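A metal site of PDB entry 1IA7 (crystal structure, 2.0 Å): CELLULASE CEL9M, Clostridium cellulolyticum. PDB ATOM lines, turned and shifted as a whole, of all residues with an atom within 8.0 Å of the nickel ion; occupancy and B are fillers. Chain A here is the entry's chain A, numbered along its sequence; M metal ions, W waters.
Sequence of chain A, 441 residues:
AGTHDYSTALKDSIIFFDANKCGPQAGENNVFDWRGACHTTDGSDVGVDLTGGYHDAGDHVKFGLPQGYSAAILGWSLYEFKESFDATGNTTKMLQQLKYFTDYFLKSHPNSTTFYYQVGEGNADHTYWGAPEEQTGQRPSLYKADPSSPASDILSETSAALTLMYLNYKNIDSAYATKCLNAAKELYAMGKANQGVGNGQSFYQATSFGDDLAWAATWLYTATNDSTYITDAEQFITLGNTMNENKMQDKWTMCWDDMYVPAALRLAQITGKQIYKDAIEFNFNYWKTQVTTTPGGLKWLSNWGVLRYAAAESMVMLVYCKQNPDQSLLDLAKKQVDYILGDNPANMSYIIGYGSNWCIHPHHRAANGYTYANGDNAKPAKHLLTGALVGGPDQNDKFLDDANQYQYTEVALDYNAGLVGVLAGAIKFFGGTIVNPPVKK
The backbone NH (N) of Asp 343 is in hydrogen-bond range of the backbone carbonyl oxygen (O) of Asp 338.
The nickel ion is bound by water W1 (2.0 Å), the side-chain carboxylate (OD2) of Asp 343 (2.0 Å), the backbone nitrogen (N) of Ala 1 (2.2 Å), a ring nitrogen (NE2) of His 4 (2.2 Å) and the backbone carbonyl oxygen (O) of Ala 1 (2.4 Å).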
ATOM      1  N   ALA A   1      18.478 -23.381  15.289  1.00  0.00           N
ATOM      2  CA  ALA A   1      17.844 -22.813  16.512  1.00  0.00           C
ATOM      3  C   ALA A   1      16.691 -23.707  16.956  1.00  0.00           C
ATOM      4  O   ALA A   1      15.985 -24.286  16.122  1.00  0.00           O
ATOM      5  CB  ALA A   1      17.326 -21.408  16.231  1.00  0.00           C
ATOM      6  N   GLY A   2      16.504 -23.817  18.268  1.00  0.00           N
ATOM      7  CA  GLY A   2      15.436 -24.650  18.793  1.00  0.00           C
ATOM      8  C   GLY A   2      14.076 -24.131  18.374  1.00  0.00           C
ATOM      9  O   GLY A   2      13.175 -24.903  18.034  1.00  0.00           O
ATOM     10  N   THR A   3      13.930 -22.810  18.378  1.00  0.00           N
ATOM     11  CA  THR A   3      12.676 -22.174  17.988  1.00  0.00           C
ATOM     12  C   THR A   3      12.908 -21.223  16.823  1.00  0.00           C
ATOM     13  O   THR A   3      13.978 -20.625  16.701  1.00  0.00           O
ATOM     14  CB  THR A   3      12.058 -21.355  19.144  1.00  0.00           C
ATOM     15  OG1 THR A   3      12.926 -20.248  19.458  1.00  0.00           O
ATOM     16  CG2 THR A   3      11.899 -22.220  20.376  1.00  0.00           C
ATOM     17  N   HIS A   4      11.899 -21.082  15.973  1.00  0.00           N
ATOM     18  CA  HIS A   4      11.984 -20.193  14.825  1.00  0.00           C
ATOM     19  C   HIS A   4      10.715 -19.345  14.739  1.00  0.00           C
ATOM     20  O   HIS A   4       9.620 -19.819  14.998  1.00  0.00           O
ATOM     21  CB  HIS A   4      12.169 -21.017  13.547  1.00  0.00           C
ATOM     22  CG  HIS A   4      13.556 -21.557  13.359  1.00  0.00           C
ATOM     23  ND1 HIS A   4      14.608 -20.764  12.943  1.00  0.00           N
ATOM     24  CD2 HIS A   4      14.075 -22.791  13.567  1.00  0.00           C
ATOM     25  CE1 HIS A   4      15.712 -21.491  12.903  1.00  0.00           C
ATOM     26  NE2 HIS A   4      15.412 -22.725  13.275  1.00  0.00           N
ATOM     27  N   TYR A   6       8.451 -18.275  12.541  1.00  0.00           N
ATOM     28  CA  TYR A   6       7.879 -18.431  11.212  1.00  0.00           C
ATOM     29  C   TYR A   6       6.866 -17.340  10.894  1.00  0.00           C
ATOM     30  O   TYR A   6       6.698 -16.944   9.740  1.00  0.00           O
ATOM     31  CB  TYR A   6       7.216 -19.806  11.071  1.00  0.00           C
ATOM     32  CG  TYR A   6       8.151 -20.974  11.282  1.00  0.00           C
ATOM     33  CD1 TYR A   6       9.289 -21.123  10.491  1.00  0.00           C
ATOM     34  CD2 TYR A   6       7.926 -21.913  12.278  1.00  0.00           C
ATOM     35  CE1 TYR A   6      10.174 -22.172  10.675  1.00  0.00           C
ATOM     36  CE2 TYR A   6       8.799 -22.982  12.479  1.00  0.00           C
ATOM     37  CZ  TYR A   6       9.924 -23.097  11.671  1.00  0.00           C
ATOM     38  OH  TYR A   6      10.804 -24.134  11.866  1.00  0.00           O
ATOM     39  N   LYS A 334      11.080 -28.811   6.940  1.00  0.00           N
ATOM     40  CA  LYS A 334      11.482 -27.969   8.048  1.00  0.00           C
ATOM     41  C   LYS A 334      12.973 -27.628   7.986  1.00  0.00           C
ATOM     42  O   LYS A 334      13.370 -26.516   8.294  1.00  0.00           O
ATOM     43  CB  LYS A 334      11.157 -28.633   9.385  1.00  0.00           C
ATOM     44  CG  LYS A 334      11.229 -27.687  10.576  1.00  0.00           C
ATOM     45  CD  LYS A 334      10.847 -28.397  11.870  1.00  0.00           C
ATOM     46  CE  LYS A 334      10.687 -27.419  13.024  1.00  0.00           C
ATOM     47  NZ  LYS A 334      11.949 -26.748  13.387  1.00  0.00           N
ATOM     48  N   LYS A 335      13.797 -28.597   7.586  1.00  0.00           N
ATOM     49  CA  LYS A 335      15.230 -28.362   7.493  1.00  0.00           C
ATOM     50  C   LYS A 335      15.563 -27.324   6.413  1.00  0.00           C
ATOM     51  O   LYS A 335      16.459 -26.496   6.602  1.00  0.00           O
ATOM     52  CB  LYS A 335      15.976 -29.670   7.205  1.00  0.00           C
ATOM     53  CG  LYS A 335      16.007 -30.627   8.400  1.00  0.00           C
ATOM     54  CD  LYS A 335      16.803 -31.889   8.081  1.00  0.00           C
ATOM     55  CE  LYS A 335      16.981 -32.756   9.325  1.00  0.00           C
ATOM     56  NZ  LYS A 335      15.683 -33.188   9.930  1.00  0.00           N
ATOM     57  N   VAL A 337      13.524 -24.920   5.296  1.00  0.00           N
ATOM     58  CA  VAL A 337      13.029 -23.628   5.747  1.00  0.00           C
ATOM     59  C   VAL A 337      13.995 -23.025   6.773  1.00  0.00           C
ATOM     60  O   VAL A 337      14.418 -21.882   6.638  1.00  0.00           O
ATOM     61  CB  VAL A 337      11.626 -23.763   6.409  1.00  0.00           C
ATOM     62  CG1 VAL A 337      11.203 -22.418   7.007  1.00  0.00           C
ATOM     63  CG2 VAL A 337      10.615 -24.219   5.381  1.00  0.00           C
ATOM     64  N   ASP A 338      14.323 -23.810   7.790  1.00  0.00           N
ATOM     65  CA  ASP A 338      15.238 -23.361   8.840  1.00  0.00           C
ATOM     66  C   ASP A 338      16.613 -22.993   8.284  1.00  0.00           C
ATOM     67  O   ASP A 338      17.280 -22.116   8.834  1.00  0.00           O
ATOM     68  CB  ASP A 338      15.367 -24.427   9.929  1.00  0.00           C
ATOM     69  CG  ASP A 338      14.061 -24.665  10.681  1.00  0.00           C
ATOM     70  OD1 ASP A 338      13.106 -23.877  10.491  1.00  0.00           O
ATOM     71  OD2 ASP A 338      13.982 -25.624  11.470  1.00  0.00           O
ATOM     72  N   TYR A 339      17.020 -23.652   7.204  1.00  0.00           N
ATOM     73  CA  TYR A 339      18.321 -23.346   6.598  1.00  0.00           C
ATOM     74  C   TYR A 339      18.219 -21.926   6.038  1.00  0.00           C
ATOM     75  O   TYR A 339      19.107 -21.099   6.232  1.00  0.00           O
ATOM     76  CB  TYR A 339      18.638 -24.345   5.468  1.00  0.00           C
ATOM     77  CG  TYR A 339      19.967 -24.101   4.763  1.00  0.00           C
ATOM     78  CD1 TYR A 339      20.119 -23.037   3.860  1.00  0.00           C
ATOM     79  CD2 TYR A 339      21.071 -24.916   4.998  1.00  0.00           C
ATOM     80  CE1 TYR A 339      21.333 -22.803   3.218  1.00  0.00           C
ATOM     81  CE2 TYR A 339      22.295 -24.691   4.353  1.00  0.00           C
ATOM     82  CZ  TYR A 339      22.424 -23.629   3.469  1.00  0.00           C
ATOM     83  OH  TYR A 339      23.636 -23.392   2.841  1.00  0.00           O
ATOM     84  N   LEU A 341      16.202 -19.604   6.936  1.00  0.00           N
ATOM     85  CA  LEU A 341      16.051 -18.667   8.049  1.00  0.00           C
ATOM     86  C   LEU A 341      17.327 -18.362   8.824  1.00  0.00           C
ATOM     87  O   LEU A 341      17.368 -17.404   9.597  1.00  0.00           O
ATOM     88  CB  LEU A 341      14.983 -19.175   9.016  1.00  0.00           C
ATOM     89  CG  LEU A 341      13.562 -19.267   8.456  1.00  0.00           C
ATOM     90  CD1 LEU A 341      12.609 -19.713   9.561  1.00  0.00           C
ATOM     91  CD2 LEU A 341      13.142 -17.922   7.889  1.00  0.00           C
ATOM     92  N   GLY A 342      18.371 -19.163   8.636  1.00  0.00           N
ATOM     93  CA  GLY A 342      19.615 -18.881   9.353  1.00  0.00           C
ATOM     94  C   GLY A 342      20.433 -20.074   9.821  1.00  0.00           C
ATOM     95  O   GLY A 342      21.593 -19.896  10.209  1.00  0.00           O
ATOM     96  N   ASP A 343      19.857 -21.270   9.802  1.00  0.00           N
ATOM     97  CA  ASP A 343      20.579 -22.475  10.228  1.00  0.00           C
ATOM     98  C   ASP A 343      21.468 -22.960   9.095  1.00  0.00           C
ATOM     99  O   ASP A 343      21.126 -23.919   8.390  1.00  0.00           O
ATOM    100  CB  ASP A 343      19.589 -23.588  10.578  1.00  0.00           C
ATOM    101  CG  ASP A 343      18.820 -23.313  11.856  1.00  0.00           C
ATOM    102  OD1 ASP A 343      18.858 -22.165  12.339  1.00  0.00           O
ATOM    103  OD2 ASP A 343      18.171 -24.254  12.364  1.00  0.00           O
ATOM    104  N   ASN A 344      22.617 -22.328   8.913  1.00  0.00           N
ATOM    105  CA  ASN A 344      23.539 -22.715   7.845  1.00  0.00           C
ATOM    106  C   ASN A 344      24.989 -22.351   8.160  1.00  0.00           C
ATOM    107  O   ASN A 344      25.255 -21.535   9.038  1.00  0.00           O
ATOM    108  CB  ASN A 344      23.096 -22.067   6.524  1.00  0.00           C
ATOM    109  CG  ASN A 344      23.014 -20.548   6.620  1.00  0.00           C
ATOM    110  OD1 ASN A 344      24.021 -19.873   6.816  1.00  0.00           O
ATOM    111  ND2 ASN A 344      21.802 -20.009   6.478  1.00  0.00           N
HETATM  112 NI    NI M   1      16.941 -24.089  13.957  1.00  0.00          NI
HETATM  113  O   HOH W   1      15.913 -25.733  13.427  1.00  0.00           O
